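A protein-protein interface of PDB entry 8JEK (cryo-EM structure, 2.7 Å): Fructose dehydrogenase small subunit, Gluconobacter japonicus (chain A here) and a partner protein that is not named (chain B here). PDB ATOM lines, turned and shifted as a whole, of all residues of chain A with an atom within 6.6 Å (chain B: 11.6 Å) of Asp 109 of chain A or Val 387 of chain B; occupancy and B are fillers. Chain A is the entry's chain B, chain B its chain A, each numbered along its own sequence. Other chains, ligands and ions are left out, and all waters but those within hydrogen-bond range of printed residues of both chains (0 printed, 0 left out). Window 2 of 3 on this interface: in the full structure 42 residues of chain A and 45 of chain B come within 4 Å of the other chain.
The side-chain carboxylate (OE2) of Glu 106 of chain A sits at hydrogen-bond distance from the backbone NH (N) of Lys 389 of chain B, at 2.8 Å. The side-chain carboxylate of Asp 392 of chain B sits at hydrogen-bond distance from the side-chain hydroxyl of Tyr 129 of chain A, at 2.5 Å.
The side-chain carboxylate (OD1) of Asp 109 of chain A is in hydrogen-bond range of a ring nitrogen (NE2) of His 118 of chain A, 2.6 Å away.
Among the printed residues, merely in contact across the chains: Val 105 of chain A with Gly 388 of chain B (3.6 Å), Glu 106 of chain A with Val 387 of chain B (3.99 Å), Glu 106 of chain A with Gly 388 of chain B (3.2 Å), Asp 109 of chain A with Val 387 of chain B (3.7 Å), Ile 125 of chain A with Val 387 of chain B (3.6 Å), Ile 125 of chain A with Leu 391 of chain B (3.8 Å), Tyr 129 of chain A with Leu 382 of chain B (3.9 Å), Tyr 129 of chain A with Leu 391 of chain B (3.9 Å) and Tyr 129 of chain A with Ile 395 of chain B (3.8 Å).
Of chain B, only Val 387 comes within 4 Å of Asp 109 of chain A. No residue of chain B comes within 4 Å of Leu 108 of chain A. No residue of chain B comes within 4 Å of Ala 110 of chain A. Ala 111 of chain A touches none of the printed residues of chain B. No residue of chain B comes within 4 Å of Met 112 of chain A. No residue of chain B comes within 4 Å of Lys 113 of chain A. No residue of chain B comes within 4 Å of Ile 122 of chain A. Of the printed residues of chain B, Ile 125 of chain A touches Val 387 and Leu 391. Of the printed residues of chain A, Leu 382 of chain B touches Tyr 129. Printed residues of chain A within 4 Å of Lys 389 of chain B: Glu 106. Printed residues of chain A within 4 Å of Ile 395 of chain B: Tyr 129 (3.8 Å). Glu 393 of chain B touches none of the printed residues of chain A. The nearest residue of chain B that does not touch Asp 109 of chain A is Gly 385 of chain B (4.8 Å). The nearest printed residue of chain B that does not touch Glu 106 of chain A is Lys 390 of chain B (4.5 Å).
Printed residues of chain B that touch a printed residue of chain A: Leu 382, Val 387, Gly 388, Lys 389, Leu 391, Asp 392 and Ile 395. Hydrophobic or aromatic side chains of chain B within 4 Å of the printed part of chain A: Leu 382, Val 387, Leu 391 and Ile 395. Along chain B the printed residues that touch a printed residue of chain A span positions 382 to 395. Hydrophobic or aromatic side chains of chain A that line the printed part of chain B: Val 105, Ile 125 and Tyr 129. Among the printed residues, no Asp or Glu carboxylate lies within 4 Å of a Lys or Arg side-chain nitrogen of the other chain.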
ATOM      1  N   ALA A  61      16.619  -1.829  26.646  1.00  0.00           N
ATOM      2  CA  ALA A  61      17.885  -1.104  26.625  1.00  0.00           C
ATOM      3  C   ALA A  61      18.902  -1.778  25.714  1.00  0.00           C
ATOM      4  O   ALA A  61      19.536  -1.121  24.880  1.00  0.00           O
ATOM      5  CB  ALA A  61      18.437  -0.979  28.044  1.00  0.00           C
ATOM      6  N   THR A  62      19.078  -3.090  25.863  1.00  0.00           N
ATOM      7  CA  THR A  62      20.028  -3.807  25.024  1.00  0.00           C
ATOM      8  C   THR A  62      19.493  -4.022  23.616  1.00  0.00           C
ATOM      9  O   THR A  62      20.278  -4.207  22.680  1.00  0.00           O
ATOM     10  CB  THR A  62      20.382  -5.150  25.662  1.00  0.00           C
ATOM     11  OG1 THR A  62      19.190  -5.921  25.841  1.00  0.00           O
ATOM     12  CG2 THR A  62      21.042  -4.938  27.012  1.00  0.00           C
ATOM     13  N   TYR A 102       9.141   5.801  23.180  1.00  0.00           N
ATOM     14  CA  TYR A 102      10.425   5.651  22.510  1.00  0.00           C
ATOM     15  C   TYR A 102      10.459   4.309  21.790  1.00  0.00           C
ATOM     16  O   TYR A 102      10.272   3.259  22.414  1.00  0.00           O
ATOM     17  CB  TYR A 102      11.568   5.759  23.516  1.00  0.00           C
ATOM     18  CG  TYR A 102      11.705   7.126  24.145  1.00  0.00           C
ATOM     19  CD1 TYR A 102      11.927   8.252  23.365  1.00  0.00           C
ATOM     20  CD2 TYR A 102      11.616   7.290  25.520  1.00  0.00           C
ATOM     21  CE1 TYR A 102      12.056   9.502  23.936  1.00  0.00           C
ATOM     22  CE2 TYR A 102      11.744   8.536  26.099  1.00  0.00           C
ATOM     23  CZ  TYR A 102      11.964   9.639  25.303  1.00  0.00           C
ATOM     24  OH  TYR A 102      12.090  10.882  25.878  1.00  0.00           O
ATOM     25  N   ASP A 104      12.987   2.682  20.313  1.00  0.00           N
ATOM     26  CA  ASP A 104      14.139   1.859  20.646  1.00  0.00           C
ATOM     27  C   ASP A 104      14.985   2.586  21.682  1.00  0.00           C
ATOM     28  O   ASP A 104      14.660   3.695  22.114  1.00  0.00           O
ATOM     29  CB  ASP A 104      14.958   1.526  19.393  1.00  0.00           C
ATOM     30  CG  ASP A 104      15.183   2.736  18.507  1.00  0.00           C
ATOM     31  OD1 ASP A 104      14.844   3.859  18.934  1.00  0.00           O
ATOM     32  OD2 ASP A 104      15.700   2.563  17.384  1.00  0.00           O
ATOM     33  N   VAL A 105      16.089   1.949  22.082  1.00  0.00           N
ATOM     34  CA  VAL A 105      16.982   2.561  23.056  1.00  0.00           C
ATOM     35  C   VAL A 105      17.746   3.735  22.463  1.00  0.00           C
ATOM     36  O   VAL A 105      18.217   4.599  23.208  1.00  0.00           O
ATOM     37  CB  VAL A 105      17.954   1.512  23.632  1.00  0.00           C
ATOM     38  CG1 VAL A 105      19.016   1.149  22.610  1.00  0.00           C
ATOM     39  CG2 VAL A 105      18.588   2.020  24.918  1.00  0.00           C
ATOM     40  N   GLU A 106      17.884   3.796  21.136  1.00  0.00           N
ATOM     41  CA  GLU A 106      18.550   4.941  20.523  1.00  0.00           C
ATOM     42  C   GLU A 106      17.773   6.227  20.771  1.00  0.00           C
ATOM     43  O   GLU A 106      18.360   7.257  21.129  1.00  0.00           O
ATOM     44  CB  GLU A 106      18.732   4.705  19.024  1.00  0.00           C
ATOM     45  CG  GLU A 106      19.835   3.719  18.673  1.00  0.00           C
ATOM     46  CD  GLU A 106      19.319   2.306  18.496  1.00  0.00           C
ATOM     47  OE1 GLU A 106      18.164   2.039  18.884  1.00  0.00           O
ATOM     48  OE2 GLU A 106      20.067   1.461  17.961  1.00  0.00           O
ATOM     49  N   ALA A 107      16.450   6.187  20.595  1.00  0.00           N
ATOM     50  CA  ALA A 107      15.633   7.371  20.836  1.00  0.00           C
ATOM     51  C   ALA A 107      15.659   7.773  22.305  1.00  0.00           C
ATOM     52  O   ALA A 107      15.764   8.963  22.627  1.00  0.00           O
ATOM     53  CB  ALA A 107      14.199   7.122  20.372  1.00  0.00           C
ATOM     54  N   LEU A 108      15.560   6.796  23.209  1.00  0.00           N
ATOM     55  CA  LEU A 108      15.621   7.095  24.636  1.00  0.00           C
ATOM     56  C   LEU A 108      16.959   7.714  25.012  1.00  0.00           C
ATOM     57  O   LEU A 108      17.009   8.689  25.771  1.00  0.00           O
ATOM     58  CB  LEU A 108      15.372   5.823  25.446  1.00  0.00           C
ATOM     59  CG  LEU A 108      15.545   5.910  26.963  1.00  0.00           C
ATOM     60  CD1 LEU A 108      14.450   6.750  27.592  1.00  0.00           C
ATOM     61  CD2 LEU A 108      15.575   4.521  27.578  1.00  0.00           C
ATOM     62  N   ASP A 109      18.057   7.164  24.490  1.00  0.00           N
ATOM     63  CA  ASP A 109      19.377   7.702  24.797  1.00  0.00           C
ATOM     64  C   ASP A 109      19.547   9.110  24.240  1.00  0.00           C
ATOM     65  O   ASP A 109      20.109   9.982  24.910  1.00  0.00           O
ATOM     66  CB  ASP A 109      20.459   6.772  24.253  1.00  0.00           C
ATOM     67  CG  ASP A 109      21.851   7.354  24.386  1.00  0.00           C
ATOM     68  OD1 ASP A 109      22.290   7.596  25.530  1.00  0.00           O
ATOM     69  OD2 ASP A 109      22.510   7.567  23.347  1.00  0.00           O
ATOM     70  N   ALA A 110      19.065   9.353  23.019  1.00  0.00           N
ATOM     71  CA  ALA A 110      19.216  10.676  22.422  1.00  0.00           C
ATOM     72  C   ALA A 110      18.354  11.719  23.121  1.00  0.00           C
ATOM     73  O   ALA A 110      18.780  12.870  23.272  1.00  0.00           O
ATOM     74  CB  ALA A 110      18.878  10.622  20.933  1.00  0.00           C
ATOM     75  N   ALA A 111      17.153  11.346  23.552  1.00  0.00           N
ATOM     76  CA  ALA A 111      16.221  12.289  24.156  1.00  0.00           C
ATOM     77  C   ALA A 111      16.357  12.388  25.670  1.00  0.00           C
ATOM     78  O   ALA A 111      15.651  13.193  26.286  1.00  0.00           O
ATOM     79  CB  ALA A 111      14.782  11.908  23.797  1.00  0.00           C
ATOM     80  N   MET A 112      17.235  11.602  26.282  1.00  0.00           N
ATOM     81  CA  MET A 112      17.389  11.592  27.734  1.00  0.00           C
ATOM     82  C   MET A 112      18.876  11.558  28.087  1.00  0.00           C
ATOM     83  O   MET A 112      19.330  10.800  28.943  1.00  0.00           O
ATOM     84  CB  MET A 112      16.598  10.424  28.331  1.00  0.00           C
ATOM     85  CG  MET A 112      16.491  10.392  29.848  1.00  0.00           C
ATOM     86  SD  MET A 112      16.534   8.722  30.528  1.00  0.00           S
ATOM     87  CE  MET A 112      18.037   8.077  29.805  1.00  0.00           C
ATOM     88  N   LYS A 113      19.661  12.394  27.403  1.00  0.00           N
ATOM     89  CA  LYS A 113      21.095  12.455  27.670  1.00  0.00           C
ATOM     90  C   LYS A 113      21.417  13.216  28.948  1.00  0.00           C
ATOM     91  O   LYS A 113      22.361  12.851  29.658  1.00  0.00           O
ATOM     92  CB  LYS A 113      21.826  13.098  26.490  1.00  0.00           C
ATOM     93  CG  LYS A 113      22.302  12.111  25.440  1.00  0.00           C
ATOM     94  CD  LYS A 113      23.288  12.748  24.477  1.00  0.00           C
ATOM     95  CE  LYS A 113      23.905  11.706  23.557  1.00  0.00           C
ATOM     96  NZ  LYS A 113      24.762  12.329  22.512  1.00  0.00           N
ATOM     97  N   ASP A 114      20.659  14.268  29.258  1.00  0.00           N
ATOM     98  CA  ASP A 114      20.964  15.126  30.395  1.00  0.00           C
ATOM     99  C   ASP A 114      20.259  14.716  31.681  1.00  0.00           C
ATOM    100  O   ASP A 114      20.611  15.228  32.748  1.00  0.00           O
ATOM    101  CB  ASP A 114      20.601  16.580  30.070  1.00  0.00           C
ATOM    102  CG  ASP A 114      21.353  17.110  28.864  1.00  0.00           C
ATOM    103  OD1 ASP A 114      22.492  16.661  28.627  1.00  0.00           O
ATOM    104  OD2 ASP A 114      20.803  17.978  28.153  1.00  0.00           O
ATOM    105  N   HIS A 118      20.147   8.682  32.943  1.00  0.00           N
ATOM    106  CA  HIS A 118      21.064   8.187  31.919  1.00  0.00           C
ATOM    107  C   HIS A 118      22.181   7.307  32.475  1.00  0.00           C
ATOM    108  O   HIS A 118      22.478   6.273  31.849  1.00  0.00           O
ATOM    109  CB  HIS A 118      21.632   9.375  31.132  1.00  0.00           C
ATOM    110  CG  HIS A 118      22.357   8.987  29.882  1.00  0.00           C
ATOM    111  ND1 HIS A 118      23.732   8.952  29.801  1.00  0.00           N
ATOM    112  CD2 HIS A 118      21.898   8.623  28.662  1.00  0.00           C
ATOM    113  CE1 HIS A 118      24.088   8.581  28.584  1.00  0.00           C
ATOM    114  NE2 HIS A 118      22.994   8.374  27.874  1.00  0.00           N
ATOM    115  N   LEU A 121      20.764   3.781  32.904  1.00  0.00           N
ATOM    116  CA  LEU A 121      20.594   3.094  31.628  1.00  0.00           C
ATOM    117  C   LEU A 121      21.931   2.594  31.096  1.00  0.00           C
ATOM    118  O   LEU A 121      22.052   1.446  30.645  1.00  0.00           O
ATOM    119  CB  LEU A 121      19.930   4.034  30.622  1.00  0.00           C
ATOM    120  CG  LEU A 121      19.755   3.538  29.188  1.00  0.00           C
ATOM    121  CD1 LEU A 121      18.651   2.502  29.111  1.00  0.00           C
ATOM    122  CD2 LEU A 121      19.473   4.702  28.254  1.00  0.00           C
ATOM    123  N   ILE A 122      22.957   3.448  31.154  1.00  0.00           N
ATOM    124  CA  ILE A 122      24.274   3.060  30.663  1.00  0.00           C
ATOM    125  C   ILE A 122      24.842   1.920  31.501  1.00  0.00           C
ATOM    126  O   ILE A 122      25.461   0.989  30.970  1.00  0.00           O
ATOM    127  CB  ILE A 122      25.209   4.281  30.643  1.00  0.00           C
ATOM    128  CG1 ILE A 122      24.792   5.246  29.532  1.00  0.00           C
ATOM    129  CG2 ILE A 122      26.651   3.854  30.449  1.00  0.00           C
ATOM    130  CD1 ILE A 122      24.874   4.652  28.147  1.00  0.00           C
ATOM    131  N   ILE A 125      23.120  -1.322  30.503  1.00  0.00           N
ATOM    132  CA  ILE A 125      23.632  -1.801  29.222  1.00  0.00           C
ATOM    133  C   ILE A 125      25.011  -2.425  29.396  1.00  0.00           C
ATOM    134  O   ILE A 125      25.289  -3.508  28.867  1.00  0.00           O
ATOM    135  CB  ILE A 125      23.658  -0.658  28.190  1.00  0.00           C
ATOM    136  CG1 ILE A 125      22.240  -0.186  27.879  1.00  0.00           C
ATOM    137  CG2 ILE A 125      24.355  -1.103  26.919  1.00  0.00           C
ATOM    138  CD1 ILE A 125      22.190   1.060  27.033  1.00  0.00           C
ATOM    139  N   TYR A 129      26.108  -6.293  28.755  1.00  0.00           N
ATOM    140  CA  TYR A 129      27.059  -6.572  27.687  1.00  0.00           C
ATOM    141  C   TYR A 129      28.359  -7.177  28.199  1.00  0.00           C
ATOM    142  O   TYR A 129      28.925  -8.050  27.537  1.00  0.00           O
ATOM    143  CB  TYR A 129      27.350  -5.297  26.896  1.00  0.00           C
ATOM    144  CG  TYR A 129      26.491  -5.150  25.663  1.00  0.00           C
ATOM    145  CD1 TYR A 129      25.175  -4.729  25.756  1.00  0.00           C
ATOM    146  CD2 TYR A 129      26.996  -5.444  24.406  1.00  0.00           C
ATOM    147  CE1 TYR A 129      24.387  -4.598  24.631  1.00  0.00           C
ATOM    148  CE2 TYR A 129      26.216  -5.320  23.277  1.00  0.00           C
ATOM    149  CZ  TYR A 129      24.913  -4.896  23.395  1.00  0.00           C
ATOM    150  OH  TYR A 129      24.134  -4.770  22.269  1.00  0.00           O
ATOM    151  N   ALA B 377      37.507  -5.145  22.157  1.00  0.00           N
ATOM    152  CA  ALA B 377      36.529  -4.423  21.353  1.00  0.00           C
ATOM    153  C   ALA B 377      35.272  -4.117  22.152  1.00  0.00           C
ATOM    154  O   ALA B 377      34.744  -3.002  22.084  1.00  0.00           O
ATOM    155  CB  ALA B 377      36.183  -5.226  20.104  1.00  0.00           C
ATOM    156  N   GLY B 378      34.780  -5.093  22.917  1.00  0.00           N
ATOM    157  CA  GLY B 378      33.605  -4.849  23.736  1.00  0.00           C
ATOM    158  C   GLY B 378      33.841  -3.776  24.778  1.00  0.00           C
ATOM    159  O   GLY B 378      33.012  -2.881  24.965  1.00  0.00           O
ATOM    160  N   MET B 379      34.985  -3.841  25.463  1.00  0.00           N
ATOM    161  CA  MET B 379      35.297  -2.842  26.480  1.00  0.00           C
ATOM    162  C   MET B 379      35.406  -1.451  25.868  1.00  0.00           C
ATOM    163  O   MET B 379      34.857  -0.478  26.403  1.00  0.00           O
ATOM    164  CB  MET B 379      36.594  -3.216  27.196  1.00  0.00           C
ATOM    165  CG  MET B 379      36.474  -4.403  28.132  1.00  0.00           C
ATOM    166  SD  MET B 379      35.635  -3.996  29.669  1.00  0.00           S
ATOM    167  CE  MET B 379      34.033  -4.716  29.365  1.00  0.00           C
ATOM    168  N   LYS B 380      36.105  -1.338  24.736  1.00  0.00           N
ATOM    169  CA  LYS B 380      36.277  -0.038  24.100  1.00  0.00           C
ATOM    170  C   LYS B 380      34.949   0.522  23.615  1.00  0.00           C
ATOM    171  O   LYS B 380      34.676   1.717  23.779  1.00  0.00           O
ATOM    172  CB  LYS B 380      37.268  -0.145  22.944  1.00  0.00           C
ATOM    173  CG  LYS B 380      37.540   1.176  22.249  1.00  0.00           C
ATOM    174  CD  LYS B 380      38.352   2.106  23.131  1.00  0.00           C
ATOM    175  CE  LYS B 380      38.803   3.335  22.367  1.00  0.00           C
ATOM    176  NZ  LYS B 380      37.662   4.216  22.011  1.00  0.00           N
ATOM    177  N   ALA B 381      34.105  -0.321  23.014  1.00  0.00           N
ATOM    178  CA  ALA B 381      32.818   0.156  22.527  1.00  0.00           C
ATOM    179  C   ALA B 381      31.890   0.537  23.671  1.00  0.00           C
ATOM    180  O   ALA B 381      31.075   1.455  23.524  1.00  0.00           O
ATOM    181  CB  ALA B 381      32.170  -0.902  21.638  1.00  0.00           C
ATOM    182  N   LEU B 382      31.986  -0.152  24.810  1.00  0.00           N
ATOM    183  CA  LEU B 382      31.209   0.255  25.974  1.00  0.00           C
ATOM    184  C   LEU B 382      31.711   1.578  26.536  1.00  0.00           C
ATOM    185  O   LEU B 382      30.922   2.390  27.031  1.00  0.00           O
ATOM    186  CB  LEU B 382      31.250  -0.834  27.045  1.00  0.00           C
ATOM    187  CG  LEU B 382      30.435  -2.097  26.767  1.00  0.00           C
ATOM    188  CD1 LEU B 382      30.624  -3.105  27.885  1.00  0.00           C
ATOM    189  CD2 LEU B 382      28.968  -1.757  26.583  1.00  0.00           C
ATOM    190  N   SER B 383      33.024   1.814  26.468  1.00  0.00           N
ATOM    191  CA  SER B 383      33.593   3.043  27.009  1.00  0.00           C
ATOM    192  C   SER B 383      33.197   4.280  26.211  1.00  0.00           C
ATOM    193  O   SER B 383      33.326   5.396  26.724  1.00  0.00           O
ATOM    194  CB  SER B 383      35.116   2.934  27.067  1.00  0.00           C
ATOM    195  OG  SER B 383      35.679   3.030  25.771  1.00  0.00           O
ATOM    196  N   MET B 384      32.721   4.116  24.981  1.00  0.00           N
ATOM    197  CA  MET B 384      32.311   5.241  24.152  1.00  0.00           C
ATOM    198  C   MET B 384      30.852   5.628  24.348  1.00  0.00           C
ATOM    199  O   MET B 384      30.378   6.557  23.685  1.00  0.00           O
ATOM    200  CB  MET B 384      32.566   4.933  22.674  1.00  0.00           C
ATOM    201  CG  MET B 384      33.970   4.446  22.376  1.00  0.00           C
ATOM    202  SD  MET B 384      34.071   3.487  20.856  1.00  0.00           S
ATOM    203  CE  MET B 384      33.971   4.787  19.633  1.00  0.00           C
ATOM    204  N   GLY B 385      30.132   4.945  25.232  1.00  0.00           N
ATOM    205  CA  GLY B 385      28.743   5.287  25.494  1.00  0.00           C
ATOM    206  C   GLY B 385      27.818   5.072  24.316  1.00  0.00           C
ATOM    207  O   GLY B 385      26.895   5.869  24.100  1.00  0.00           O
ATOM    208  N   LEU B 386      28.044   4.013  23.547  1.00  0.00           N
ATOM    209  CA  LEU B 386      27.185   3.676  22.423  1.00  0.00           C
ATOM    210  C   LEU B 386      26.054   2.766  22.882  1.00  0.00           C
ATOM    211  O   LEU B 386      26.205   1.980  23.821  1.00  0.00           O
ATOM    212  CB  LEU B 386      27.987   2.997  21.312  1.00  0.00           C
ATOM    213  CG  LEU B 386      29.010   3.876  20.593  1.00  0.00           C
ATOM    214  CD1 LEU B 386      30.033   3.022  19.873  1.00  0.00           C
ATOM    215  CD2 LEU B 386      28.320   4.814  19.623  1.00  0.00           C
ATOM    216  N   VAL B 387      24.906   2.888  22.215  1.00  0.00           N
ATOM    217  CA  VAL B 387      23.721   2.113  22.551  1.00  0.00           C
ATOM    218  C   VAL B 387      23.126   1.527  21.278  1.00  0.00           C
ATOM    219  O   VAL B 387      23.346   2.024  20.171  1.00  0.00           O
ATOM    220  CB  VAL B 387      22.659   2.955  23.292  1.00  0.00           C
ATOM    221  CG1 VAL B 387      23.232   3.544  24.570  1.00  0.00           C
ATOM    222  CG2 VAL B 387      22.126   4.052  22.387  1.00  0.00           C
ATOM    223  N   GLY B 388      22.364   0.449  21.453  1.00  0.00           N
ATOM    224  CA  GLY B 388      21.582  -0.089  20.353  1.00  0.00           C
ATOM    225  C   GLY B 388      22.435  -0.742  19.283  1.00  0.00           C
ATOM    226  O   GLY B 388      23.411  -1.445  19.566  1.00  0.00           O
ATOM    227  N   LYS B 389      22.048  -0.513  18.026  1.00  0.00           N
ATOM    228  CA  LYS B 389      22.724  -1.160  16.905  1.00  0.00           C
ATOM    229  C   LYS B 389      24.145  -0.639  16.733  1.00  0.00           C
ATOM    230  O   LYS B 389      25.038  -1.389  16.327  1.00  0.00           O
ATOM    231  CB  LYS B 389      21.920  -0.953  15.623  1.00  0.00           C
ATOM    232  CG  LYS B 389      20.595  -1.690  15.600  1.00  0.00           C
ATOM    233  CD  LYS B 389      19.949  -1.622  14.230  1.00  0.00           C
ATOM    234  CE  LYS B 389      18.541  -2.189  14.261  1.00  0.00           C
ATOM    235  NZ  LYS B 389      18.530  -3.623  14.659  1.00  0.00           N
ATOM    236  N   LYS B 390      24.367   0.645  17.022  1.00  0.00           N
ATOM    237  CA  LYS B 390      25.702   1.215  16.881  1.00  0.00           C
ATOM    238  C   LYS B 390      26.699   0.539  17.810  1.00  0.00           C
ATOM    239  O   LYS B 390      27.863   0.353  17.440  1.00  0.00           O
ATOM    240  CB  LYS B 390      25.664   2.718  17.144  1.00  0.00           C
ATOM    241  CG  LYS B 390      24.732   3.479  16.219  1.00  0.00           C
ATOM    242  CD  LYS B 390      25.149   3.311  14.769  1.00  0.00           C
ATOM    243  CE  LYS B 390      24.168   3.982  13.826  1.00  0.00           C
ATOM    244  NZ  LYS B 390      24.462   3.660  12.402  1.00  0.00           N
ATOM    245  N   LEU B 391      26.262   0.157  19.013  1.00  0.00           N
ATOM    246  CA  LEU B 391      27.142  -0.557  19.932  1.00  0.00           C
ATOM    247  C   LEU B 391      27.593  -1.885  19.336  1.00  0.00           C
ATOM    248  O   LEU B 391      28.787  -2.212  19.348  1.00  0.00           O
ATOM    249  CB  LEU B 391      26.426  -0.777  21.265  1.00  0.00           C
ATOM    250  CG  LEU B 391      27.180  -1.480  22.393  1.00  0.00           C
ATOM    251  CD1 LEU B 391      28.603  -0.971  22.496  1.00  0.00           C
ATOM    252  CD2 LEU B 391      26.453  -1.296  23.709  1.00  0.00           C
ATOM    253  N   ASP B 392      26.650  -2.660  18.796  1.00  0.00           N
ATOM    254  CA  ASP B 392      26.993  -3.948  18.204  1.00  0.00           C
ATOM    255  C   ASP B 392      27.886  -3.775  16.984  1.00  0.00           C
ATOM    256  O   ASP B 392      28.832  -4.548  16.781  1.00  0.00           O
ATOM    257  CB  ASP B 392      25.722  -4.707  17.829  1.00  0.00           C
ATOM    258  CG  ASP B 392      24.862  -5.030  19.028  1.00  0.00           C
ATOM    259  OD1 ASP B 392      25.415  -5.183  20.135  1.00  0.00           O
ATOM    260  OD2 ASP B 392      23.630  -5.131  18.862  1.00  0.00           O
ATOM    261  N   GLU B 393      27.593  -2.774  16.152  1.00  0.00           N
ATOM    262  CA  GLU B 393      28.421  -2.520  14.980  1.00  0.00           C
ATOM    263  C   GLU B 393      29.843  -2.155  15.383  1.00  0.00           C
ATOM    264  O   GLU B 393      30.807  -2.629  14.775  1.00  0.00           O
ATOM    265  CB  GLU B 393      27.808  -1.410  14.129  1.00  0.00           C
ATOM    266  CG  GLU B 393      26.490  -1.777  13.480  1.00  0.00           C
ATOM    267  CD  GLU B 393      25.855  -0.604  12.766  1.00  0.00           C
ATOM    268  OE1 GLU B 393      26.508   0.456  12.668  1.00  0.00           O
ATOM    269  OE2 GLU B 393      24.703  -0.739  12.305  1.00  0.00           O
ATOM    270  N   GLU B 394      29.991  -1.317  16.410  1.00  0.00           N
ATOM    271  CA  GLU B 394      31.320  -0.947  16.880  1.00  0.00           C
ATOM    272  C   GLU B 394      32.061  -2.155  17.438  1.00  0.00           C
ATOM    273  O   GLU B 394      33.252  -2.339  17.172  1.00  0.00           O
ATOM    274  CB  GLU B 394      31.215   0.157  17.932  1.00  0.00           C
ATOM    275  CG  GLU B 394      32.549   0.744  18.351  1.00  0.00           C
ATOM    276  CD  GLU B 394      33.131   1.688  17.317  1.00  0.00           C
ATOM    277  OE1 GLU B 394      32.503   1.887  16.258  1.00  0.00           O
ATOM    278  OE2 GLU B 394      34.226   2.232  17.565  1.00  0.00           O
ATOM    279  N   ILE B 395      31.368  -2.992  18.214  1.00  0.00           N
ATOM    280  CA  ILE B 395      32.015  -4.179  18.768  1.00  0.00           C
ATOM    281  C   ILE B 395      32.504  -5.089  17.649  1.00  0.00           C
ATOM    282  O   ILE B 395      33.648  -5.559  17.669  1.00  0.00           O
ATOM    283  CB  ILE B 395      31.064  -4.926  19.721  1.00  0.00           C
ATOM    284  CG1 ILE B 395      30.711  -4.057  20.926  1.00  0.00           C
ATOM    285  CG2 ILE B 395      31.692  -6.231  20.178  1.00  0.00           C
ATOM    286  CD1 ILE B 395      29.664  -4.661  21.828  1.00  0.00           C
ATOM    287  N   ARG B 397      33.139  -4.318  14.459  1.00  0.00           N
ATOM    288  CA  ARG B 397      34.193  -3.678  13.680  1.00  0.00           C
ATOM    289  C   ARG B 397      35.528  -3.712  14.412  1.00  0.00           C
ATOM    290  O   ARG B 397      36.567  -4.001  13.809  1.00  0.00           O
ATOM    291  CB  ARG B 397      33.798  -2.238  13.358  1.00  0.00           C
ATOM    292  CG  ARG B 397      34.339  -1.720  12.040  1.00  0.00           C
ATOM    293  CD  ARG B 397      34.279  -0.199  11.967  1.00  0.00           C
ATOM    294  NE  ARG B 397      33.388   0.380  12.965  1.00  0.00           N
ATOM    295  CZ  ARG B 397      32.104   0.652  12.761  1.00  0.00           C
ATOM    296  NH1 ARG B 397      31.520   0.398  11.602  1.00  0.00           N
ATOM    297  NH2 ARG B 397      31.390   1.190  13.744  1.00  0.00           N
